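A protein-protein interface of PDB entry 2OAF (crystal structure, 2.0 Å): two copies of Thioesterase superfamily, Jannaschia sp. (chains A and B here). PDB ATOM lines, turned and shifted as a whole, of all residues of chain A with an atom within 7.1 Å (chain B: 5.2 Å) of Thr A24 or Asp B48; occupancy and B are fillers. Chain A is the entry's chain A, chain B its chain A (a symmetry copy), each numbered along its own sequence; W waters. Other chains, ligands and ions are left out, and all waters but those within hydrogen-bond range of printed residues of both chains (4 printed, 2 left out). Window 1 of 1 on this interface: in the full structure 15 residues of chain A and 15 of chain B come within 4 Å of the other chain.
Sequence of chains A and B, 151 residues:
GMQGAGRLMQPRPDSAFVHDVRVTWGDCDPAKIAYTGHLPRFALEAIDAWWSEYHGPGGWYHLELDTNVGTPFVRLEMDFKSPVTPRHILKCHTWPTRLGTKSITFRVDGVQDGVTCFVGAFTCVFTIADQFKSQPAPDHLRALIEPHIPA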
ATOM      1  N   VAL A  21      13.260 -10.942 -23.131  1.00  0.00           N
ATOM      2  CA  VAL A  21      13.617  -9.615 -22.660  1.00  0.00           C
ATOM      3  C   VAL A  21      13.505  -9.654 -21.148  1.00  0.00           C
ATOM      4  O   VAL A  21      12.460 -10.054 -20.595  1.00  0.00           O
ATOM      5  CB  VAL A  21      12.676  -8.524 -23.208  1.00  0.00           C
ATOM      6  CG1 VAL A  21      12.913  -7.182 -22.501  1.00  0.00           C
ATOM      7  CG2 VAL A  21      12.828  -8.382 -24.718  1.00  0.00           C
ATOM      8  N   ARG A  22      14.582  -9.266 -20.465  1.00  0.00           N
ATOM      9  CA  ARG A  22      14.533  -9.173 -19.022  1.00  0.00           C
ATOM     10  C   ARG A  22      14.065  -7.764 -18.624  1.00  0.00           C
ATOM     11  O   ARG A  22      14.712  -6.753 -18.950  1.00  0.00           O
ATOM     12  CB  ARG A  22      15.870  -9.539 -18.377  1.00  0.00           C
ATOM     13  CG  ARG A  22      15.739  -9.764 -16.861  1.00  0.00           C
ATOM     14  CD  ARG A  22      16.970 -10.392 -16.284  1.00  0.00           C
ATOM     15  NE  ARG A  22      17.071 -11.813 -16.605  1.00  0.00           N
ATOM     16  CZ  ARG A  22      16.944 -12.815 -15.734  1.00  0.00           C
ATOM     17  NH1 ARG A  22      16.715 -12.584 -14.440  1.00  0.00           N
ATOM     18  NH2 ARG A  22      17.060 -14.070 -16.163  1.00  0.00           N
ATOM     19  N   VAL A  23      12.906  -7.698 -17.971  1.00  0.00           N
ATOM     20  CA  VAL A  23      12.309  -6.424 -17.589  1.00  0.00           C
ATOM     21  C   VAL A  23      12.744  -6.176 -16.157  1.00  0.00           C
ATOM     22  O   VAL A  23      12.735  -7.087 -15.342  1.00  0.00           O
ATOM     23  CB  VAL A  23      10.782  -6.456 -17.700  1.00  0.00           C
ATOM     24  CG1 VAL A  23      10.170  -5.099 -17.282  1.00  0.00           C
ATOM     25  CG2 VAL A  23      10.391  -6.847 -19.123  1.00  0.00           C
ATOM     26  N   THR A  24      13.174  -4.948 -15.863  1.00  0.00           N
ATOM     27  CA  THR A  24      13.610  -4.636 -14.539  1.00  0.00           C
ATOM     28  C   THR A  24      12.931  -3.424 -13.936  1.00  0.00           C
ATOM     29  O   THR A  24      12.135  -2.711 -14.582  1.00  0.00           O
ATOM     30  CB  THR A  24      15.119  -4.372 -14.526  1.00  0.00           C
ATOM     31  OG1 THR A  24      15.379  -3.191 -15.259  1.00  0.00           O
ATOM     32  CG2 THR A  24      15.910  -5.552 -15.111  1.00  0.00           C
ATOM     33  N   TRP A  25      13.264  -3.220 -12.670  1.00  0.00           N
ATOM     34  CA  TRP A  25      12.891  -2.054 -11.896  1.00  0.00           C
ATOM     35  C   TRP A  25      12.972  -0.769 -12.665  1.00  0.00           C
ATOM     36  O   TRP A  25      11.995  -0.013 -12.672  1.00  0.00           O
ATOM     37  CB  TRP A  25      13.783  -1.996 -10.651  1.00  0.00           C
ATOM     38  CG  TRP A  25      13.690  -0.814  -9.817  1.00  0.00           C
ATOM     39  CD1 TRP A  25      14.578   0.229  -9.793  1.00  0.00           C
ATOM     40  CD2 TRP A  25      12.736  -0.546  -8.792  1.00  0.00           C
ATOM     41  NE1 TRP A  25      14.205   1.141  -8.845  1.00  0.00           N
ATOM     42  CE2 TRP A  25      13.087   0.685  -8.205  1.00  0.00           C
ATOM     43  CE3 TRP A  25      11.623  -1.224  -8.305  1.00  0.00           C
ATOM     44  CZ2 TRP A  25      12.361   1.252  -7.172  1.00  0.00           C
ATOM     45  CZ3 TRP A  25      10.893  -0.656  -7.305  1.00  0.00           C
ATOM     46  CH2 TRP A  25      11.275   0.565  -6.729  1.00  0.00           C
ATOM     47  N   GLY A  26      14.081  -0.547 -13.339  1.00  0.00           N
ATOM     48  CA  GLY A  26      14.323   0.715 -14.026  1.00  0.00           C
ATOM     49  C   GLY A  26      13.537   0.901 -15.310  1.00  0.00           C
ATOM     50  O   GLY A  26      13.482   2.000 -15.819  1.00  0.00           O
ATOM     51  N   ASP A  27      12.924  -0.165 -15.812  1.00  0.00           N
ATOM     52  CA  ASP A  27      11.993  -0.083 -16.926  1.00  0.00           C
ATOM     53  C   ASP A  27      10.609   0.318 -16.487  1.00  0.00           C
ATOM     54  O   ASP A  27       9.754   0.593 -17.336  1.00  0.00           O
ATOM     55  CB  ASP A  27      11.885  -1.425 -17.589  1.00  0.00           C
ATOM     56  CG  ASP A  27      13.184  -1.862 -18.206  1.00  0.00           C
ATOM     57  OD1 ASP A  27      13.885  -1.020 -18.839  1.00  0.00           O
ATOM     58  OD2 ASP A  27      13.489  -3.062 -18.088  1.00  0.00           O
ATOM     59  N   CYS A  28      10.371   0.338 -15.173  1.00  0.00           N
ATOM     60  CA  CYS A  28       9.022   0.558 -14.615  1.00  0.00           C
ATOM     61  C   CYS A  28       8.779   1.982 -14.126  1.00  0.00           C
ATOM     62  O   CYS A  28       9.681   2.642 -13.619  1.00  0.00           O
ATOM     63  CB  CYS A  28       8.755  -0.415 -13.456  1.00  0.00           C
ATOM     64  SG  CYS A  28       8.801  -2.189 -13.897  1.00  0.00           S
ATOM     65  N   ASP A  29       7.539   2.443 -14.283  1.00  0.00           N
ATOM     66  CA  ASP A  29       7.143   3.767 -13.881  1.00  0.00           C
ATOM     67  C   ASP A  29       6.496   3.705 -12.491  1.00  0.00           C
ATOM     68  O   ASP A  29       6.403   2.626 -11.877  1.00  0.00           O
ATOM     69  CB  ASP A  29       6.241   4.391 -14.934  1.00  0.00           C
ATOM     70  CG  ASP A  29       4.905   3.664 -15.103  1.00  0.00           C
ATOM     71  OD1 ASP A  29       4.489   2.933 -14.178  1.00  0.00           O
ATOM     72  OD2 ASP A  29       4.276   3.849 -16.174  1.00  0.00           O
ATOM     73  N   ILE A  33       4.632  -0.778 -13.235  1.00  0.00           N
ATOM     74  CA  ILE A  33       4.597  -1.570 -14.461  1.00  0.00           C
ATOM     75  C   ILE A  33       5.539  -0.918 -15.460  1.00  0.00           C
ATOM     76  O   ILE A  33       5.927   0.248 -15.291  1.00  0.00           O
ATOM     77  CB  ILE A  33       3.136  -1.657 -15.076  1.00  0.00           C
ATOM     78  CG1 ILE A  33       2.635  -0.270 -15.528  1.00  0.00           C
ATOM     79  CG2 ILE A  33       2.142  -2.311 -14.069  1.00  0.00           C
ATOM     80  CD1 ILE A  33       1.296  -0.300 -16.320  1.00  0.00           C
ATOM     81  N   ALA A  34       5.892  -1.669 -16.497  1.00  0.00           N
ATOM     82  CA  ALA A  34       6.820  -1.197 -17.527  1.00  0.00           C
ATOM     83  C   ALA A  34       6.261   0.075 -18.153  1.00  0.00           C
ATOM     84  O   ALA A  34       5.111   0.109 -18.527  1.00  0.00           O
ATOM     85  CB  ALA A  34       6.992  -2.246 -18.567  1.00  0.00           C
ATOM     86  N   PHE A  42      11.463  -2.744 -26.632  1.00  0.00           N
ATOM     87  CA  PHE A  42      11.554  -4.192 -26.418  1.00  0.00           C
ATOM     88  C   PHE A  42      11.163  -4.959 -27.693  1.00  0.00           C
ATOM     89  O   PHE A  42      11.838  -5.892 -28.102  1.00  0.00           O
ATOM     90  CB  PHE A  42      10.620  -4.624 -25.311  1.00  0.00           C
ATOM     91  CG  PHE A  42      10.963  -4.087 -23.945  1.00  0.00           C
ATOM     92  CD1 PHE A  42      12.236  -3.644 -23.622  1.00  0.00           C
ATOM     93  CD2 PHE A  42       9.972  -4.074 -22.947  1.00  0.00           C
ATOM     94  CE1 PHE A  42      12.527  -3.154 -22.317  1.00  0.00           C
ATOM     95  CE2 PHE A  42      10.248  -3.592 -21.651  1.00  0.00           C
ATOM     96  CZ  PHE A  42      11.536  -3.134 -21.347  1.00  0.00           C
ATOM     97  N   THR A  85       5.739  -6.617 -16.204  1.00  0.00           N
ATOM     98  CA  THR A  85       6.472  -6.390 -14.970  1.00  0.00           C
ATOM     99  C   THR A  85       7.751  -7.239 -14.901  1.00  0.00           C
ATOM    100  O   THR A  85       7.938  -8.192 -15.686  1.00  0.00           O
ATOM    101  CB  THR A  85       5.599  -6.724 -13.724  1.00  0.00           C
ATOM    102  OG1 THR A  85       5.538  -8.143 -13.563  1.00  0.00           O
ATOM    103  CG2 THR A  85       4.202  -6.143 -13.791  1.00  0.00           C
ATOM    104  N   PRO A  86       8.636  -6.915 -13.950  1.00  0.00           N
ATOM    105  CA  PRO A  86       9.834  -7.716 -13.738  1.00  0.00           C
ATOM    106  C   PRO A  86       9.616  -9.094 -13.136  1.00  0.00           C
ATOM    107  O   PRO A  86      10.579  -9.823 -12.937  1.00  0.00           O
ATOM    108  CB  PRO A  86      10.684  -6.849 -12.811  1.00  0.00           C
ATOM    109  CG  PRO A  86      10.087  -5.478 -12.865  1.00  0.00           C
ATOM    110  CD  PRO A  86       8.631  -5.692 -13.133  1.00  0.00           C
ATOM    111  N   LEU B  44      23.650  -1.604 -14.459  1.00  0.00           N
ATOM    112  CA  LEU B  44      22.636  -1.654 -13.419  1.00  0.00           C
ATOM    113  C   LEU B  44      21.690  -2.819 -13.644  1.00  0.00           C
ATOM    114  O   LEU B  44      21.223  -3.405 -12.676  1.00  0.00           O
ATOM    115  CB  LEU B  44      21.886  -0.324 -13.296  1.00  0.00           C
ATOM    116  CG  LEU B  44      22.341   0.677 -12.225  1.00  0.00           C
ATOM    117  CD1 LEU B  44      23.807   0.936 -12.248  1.00  0.00           C
ATOM    118  CD2 LEU B  44      21.584   1.951 -12.511  1.00  0.00           C
ATOM    119  N   GLU B  45      21.428  -3.148 -14.909  1.00  0.00           N
ATOM    120  CA  GLU B  45      20.648  -4.336 -15.267  1.00  0.00           C
ATOM    121  C   GLU B  45      21.329  -5.606 -14.751  1.00  0.00           C
ATOM    122  O   GLU B  45      20.668  -6.539 -14.295  1.00  0.00           O
ATOM    123  CB  GLU B  45      20.412  -4.391 -16.803  1.00  0.00           C
ATOM    124  CG  GLU B  45      19.433  -3.299 -17.304  1.00  0.00           C
ATOM    125  CD  GLU B  45      19.279  -3.156 -18.844  1.00  0.00           C
ATOM    126  OE1 GLU B  45      19.964  -3.835 -19.664  1.00  0.00           O
ATOM    127  OE2 GLU B  45      18.416  -2.331 -19.219  1.00  0.00           O
ATOM    128  N   ALA B  46      22.656  -5.638 -14.836  1.00  0.00           N
ATOM    129  CA  ALA B  46      23.460  -6.765 -14.342  1.00  0.00           C
ATOM    130  C   ALA B  46      23.363  -6.906 -12.824  1.00  0.00           C
ATOM    131  O   ALA B  46      23.242  -8.019 -12.322  1.00  0.00           O
ATOM    132  CB  ALA B  46      24.917  -6.623 -14.792  1.00  0.00           C
ATOM    133  N   ILE B  47      23.435  -5.786 -12.096  1.00  0.00           N
ATOM    134  CA  ILE B  47      23.258  -5.783 -10.624  1.00  0.00           C
ATOM    135  C   ILE B  47      21.832  -6.267 -10.248  1.00  0.00           C
ATOM    136  O   ILE B  47      21.654  -7.091  -9.355  1.00  0.00           O
ATOM    137  CB  ILE B  47      23.535  -4.371 -10.013  1.00  0.00           C
ATOM    138  CG1 ILE B  47      24.986  -3.952 -10.289  1.00  0.00           C
ATOM    139  CG2 ILE B  47      23.280  -4.358  -8.496  1.00  0.00           C
ATOM    140  CD1 ILE B  47      25.343  -2.493  -9.934  1.00  0.00           C
ATOM    141  N   ASP B  48      20.822  -5.781 -10.962  1.00  0.00           N
ATOM    142  CA  ASP B  48      19.464  -6.271 -10.725  1.00  0.00           C
ATOM    143  C   ASP B  48      19.395  -7.778 -10.971  1.00  0.00           C
ATOM    144  O   ASP B  48      18.775  -8.493 -10.185  1.00  0.00           O
ATOM    145  CB  ASP B  48      18.431  -5.546 -11.589  1.00  0.00           C
ATOM    146  CG  ASP B  48      17.024  -6.159 -11.474  1.00  0.00           C
ATOM    147  OD1 ASP B  48      16.758  -7.182 -12.156  1.00  0.00           O
ATOM    148  OD2 ASP B  48      16.196  -5.607 -10.705  1.00  0.00           O
ATOM    149  N   ALA B  49      20.051  -8.263 -12.020  1.00  0.00           N
ATOM    150  CA  ALA B  49      20.089  -9.690 -12.297  1.00  0.00           C
ATOM    151  C   ALA B  49      20.807 -10.431 -11.181  1.00  0.00           C
ATOM    152  O   ALA B  49      20.481 -11.571 -10.876  1.00  0.00           O
ATOM    153  CB  ALA B  49      20.748  -9.952 -13.678  1.00  0.00           C
ATOM    154  N   TRP B  50      21.796  -9.783 -10.575  1.00  0.00           N
ATOM    155  CA  TRP B  50      22.520 -10.376  -9.447  1.00  0.00           C
ATOM    156  C   TRP B  50      21.575 -10.611  -8.266  1.00  0.00           C
ATOM    157  O   TRP B  50      21.535 -11.677  -7.685  1.00  0.00           O
ATOM    158  CB  TRP B  50      23.672  -9.454  -9.023  1.00  0.00           C
ATOM    159  CG  TRP B  50      24.580 -10.114  -8.045  1.00  0.00           C
ATOM    160  CD1 TRP B  50      25.728 -10.792  -8.320  1.00  0.00           C
ATOM    161  CD2 TRP B  50      24.402 -10.175  -6.627  1.00  0.00           C
ATOM    162  NE1 TRP B  50      26.277 -11.259  -7.160  1.00  0.00           N
ATOM    163  CE2 TRP B  50      25.497 -10.875  -6.102  1.00  0.00           C
ATOM    164  CE3 TRP B  50      23.434  -9.682  -5.749  1.00  0.00           C
ATOM    165  CZ2 TRP B  50      25.623 -11.161  -4.737  1.00  0.00           C
ATOM    166  CZ3 TRP B  50      23.570  -9.959  -4.375  1.00  0.00           C
ATOM    167  CH2 TRP B  50      24.671 -10.685  -3.897  1.00  0.00           C
ATOM    168  N   TRP B  51      20.779  -9.605  -7.937  1.00  0.00           N
ATOM    169  CA  TRP B  51      19.773  -9.753  -6.889  1.00  0.00           C
ATOM    170  C   TRP B  51      18.783 -10.848  -7.222  1.00  0.00           C
ATOM    171  O   TRP B  51      18.395 -11.614  -6.353  1.00  0.00           O
ATOM    172  CB  TRP B  51      19.012  -8.434  -6.654  1.00  0.00           C
ATOM    173  CG  TRP B  51      19.809  -7.440  -5.931  1.00  0.00           C
ATOM    174  CD1 TRP B  51      20.393  -6.333  -6.461  1.00  0.00           C
ATOM    175  CD2 TRP B  51      20.147  -7.444  -4.550  1.00  0.00           C
ATOM    176  NE1 TRP B  51      21.064  -5.632  -5.500  1.00  0.00           N
ATOM    177  CE2 TRP B  51      20.928  -6.282  -4.309  1.00  0.00           C
ATOM    178  CE3 TRP B  51      19.857  -8.288  -3.480  1.00  0.00           C
ATOM    179  CZ2 TRP B  51      21.421  -5.956  -3.048  1.00  0.00           C
ATOM    180  CZ3 TRP B  51      20.350  -7.955  -2.227  1.00  0.00           C
ATOM    181  CH2 TRP B  51      21.121  -6.808  -2.025  1.00  0.00           C
ATOM    182  N   SER B  52      18.361 -10.925  -8.481  1.00  0.00           N
ATOM    183  CA  SER B  52      17.465 -12.016  -8.897  1.00  0.00           C
ATOM    184  C   SER B  52      18.075 -13.399  -8.631  1.00  0.00           C
ATOM    185  O   SER B  52      17.405 -14.326  -8.150  1.00  0.00           O
ATOM    186  CB  SER B  52      17.115 -11.878 -10.366  1.00  0.00           C
ATOM    187  OG  SER B  52      16.151 -10.857 -10.523  1.00  0.00           O
ATOM    188  N   GLY B  58      12.788 -11.334  -9.779  1.00  0.00           N
ATOM    189  CA  GLY B  58      12.243  -9.995  -9.776  1.00  0.00           C
ATOM    190  C   GLY B  58      13.221  -8.945  -9.306  1.00  0.00           C
ATOM    191  O   GLY B  58      12.859  -7.762  -9.251  1.00  0.00           O
ATOM    192  N   GLY B  59      14.455  -9.346  -8.959  1.00  0.00           N
ATOM    193  CA  GLY B  59      15.517  -8.353  -8.720  1.00  0.00           C
ATOM    194  C   GLY B  59      15.106  -7.247  -7.752  1.00  0.00           C
ATOM    195  O   GLY B  59      14.481  -7.556  -6.722  1.00  0.00           O
ATOM    196  N   TRP B  60      15.443  -5.982  -8.080  1.00  0.00           N
ATOM    197  CA  TRP B  60      15.092  -4.847  -7.241  1.00  0.00           C
ATOM    198  C   TRP B  60      13.614  -4.681  -7.034  1.00  0.00           C
ATOM    199  O   TRP B  60      13.187  -4.264  -5.967  1.00  0.00           O
ATOM    200  CB  TRP B  60      15.626  -3.523  -7.809  1.00  0.00           C
ATOM    201  CG  TRP B  60      17.061  -3.300  -7.595  1.00  0.00           C
ATOM    202  CD1 TRP B  60      17.779  -3.538  -6.450  1.00  0.00           C
ATOM    203  CD2 TRP B  60      17.980  -2.752  -8.539  1.00  0.00           C
ATOM    204  NE1 TRP B  60      19.107  -3.173  -6.638  1.00  0.00           N
ATOM    205  CE2 TRP B  60      19.255  -2.704  -7.914  1.00  0.00           C
ATOM    206  CE3 TRP B  60      17.860  -2.322  -9.862  1.00  0.00           C
ATOM    207  CZ2 TRP B  60      20.382  -2.236  -8.568  1.00  0.00           C
ATOM    208  CZ3 TRP B  60      18.966  -1.847 -10.498  1.00  0.00           C
ATOM    209  CH2 TRP B  60      20.220  -1.805  -9.861  1.00  0.00           C
ATOM    210  N   TYR B  61      12.815  -4.988  -8.051  1.00  0.00           N
ATOM    211  CA  TYR B  61      11.368  -4.853  -7.951  1.00  0.00           C
ATOM    212  C   TYR B  61      10.830  -5.714  -6.820  1.00  0.00           C
ATOM    213  O   TYR B  61      10.056  -5.258  -5.976  1.00  0.00           O
ATOM    214  CB  TYR B  61      10.766  -5.248  -9.299  1.00  0.00           C
ATOM    215  CG  TYR B  61       9.307  -5.042  -9.499  1.00  0.00           C
ATOM    216  CD1 TYR B  61       8.396  -6.038  -9.190  1.00  0.00           C
ATOM    217  CD2 TYR B  61       8.837  -3.892 -10.107  1.00  0.00           C
ATOM    218  CE1 TYR B  61       7.033  -5.871  -9.442  1.00  0.00           C
ATOM    219  CE2 TYR B  61       7.488  -3.704 -10.346  1.00  0.00           C
ATOM    220  CZ  TYR B  61       6.597  -4.698 -10.033  1.00  0.00           C
ATOM    221  OH  TYR B  61       5.291  -4.488 -10.293  1.00  0.00           O
HETATM  222  O   HOH W   1      19.332 -13.040 -12.900  1.00  0.00           O
HETATM  223  O   HOH W   2      15.817  -2.242 -20.510  1.00  0.00           O
HETATM  224  O   HOH W   3      17.035  -0.992 -17.038  1.00  0.00           O
HETATM  225  O   HOH W   4      16.342  -9.774 -13.040  1.00  0.00           O
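Water W4 lies within hydrogen-bond range of OG of Ser B52 (2.7 Å), OD1 of Asp B48 (2.8 Å) and NH1 of Arg A22 (3.2 Å). Water W1 lies within hydrogen-bond range of the backbone carbonyl oxygen (O) of Ala B49 and the guanidinium group (NH1) of Arg A22. Water W2 lies within hydrogen-bond range of OD1 of Asp A27 (2.8 Å) and OE2 of Glu B45 (2.9 Å). Water W3 bridges OE2 of Glu B45 (2.9 Å) and OG1 of Thr A24 (3.3 Å).
No position is printed for both chains. Of the 5 pairs that touch across the chains among the printed residues, none has its exchanged pair printed and touching as well.
Among the printed residues, merely in contact across the chains: Pro A86 with Tyr B61 (3.4 Å), Thr A24 with Asp B48 (3.5 Å), Pro A86 with Gly B58 (3.6 Å), Trp A25 with Tyr B61 (3.7 Å) and Trp A25 with Trp B60 (3.7 Å).
Printed residues of chain B within 4 Å of Thr A24: Asp B48 (3.5 Å). Printed residues of chain A within 4 Å of Gly B58: Pro A86 (3.6 Å). Printed residues of chain A within 4 Å of Trp B60: Trp A25 (3.7 Å). Of the printed residues of chain B, Trp A25 touches Trp B60 and Tyr B61. Printed residues of chain A within 4 Å of Tyr B61: Trp A25 (3.7 Å) and Pro A86 (3.4 Å). Asp A27 touches none of the printed residues of chain B. The nearest printed residue of chain B that does not touch Thr A24 is Glu B45 (4.5 Å). The nearest printed residue of chain B that does not touch Pro A86 is Gly B59 (5.6 Å).
OG of Ser B52 lies within hydrogen-bond range of N of Gly B58, at 3.5 Å. N of Thr A24 lies within hydrogen-bond range of OD2 of Asp A27. The side-chain carboxylate of Asp B48 lies within hydrogen-bond range of the backbone NH of Trp B60 (2.8 Å). O of Thr A24 lies within hydrogen-bond range of SG of Cys A28 (3.4 Å).
Printed residues of chain B that touch a printed residue of chain A: Asp B48, Gly B58, Trp B60 and Tyr B61. Of the 14 printed residues of chain A, 3 touch a printed residue of chain B. Printed residues of chain A that touch a printed residue of chain B: Thr A24, Trp A25 and Pro A86. Hydrophobic or aromatic side chains of chain A that line the printed part of chain B: Trp A25 and Pro A86. Among the printed residues, 5 pairs touch across the chains. Among the printed residues, no Asp or Glu carboxylate lies within 4 Å of a Lys or Arg side-chain nitrogen of the other chain.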
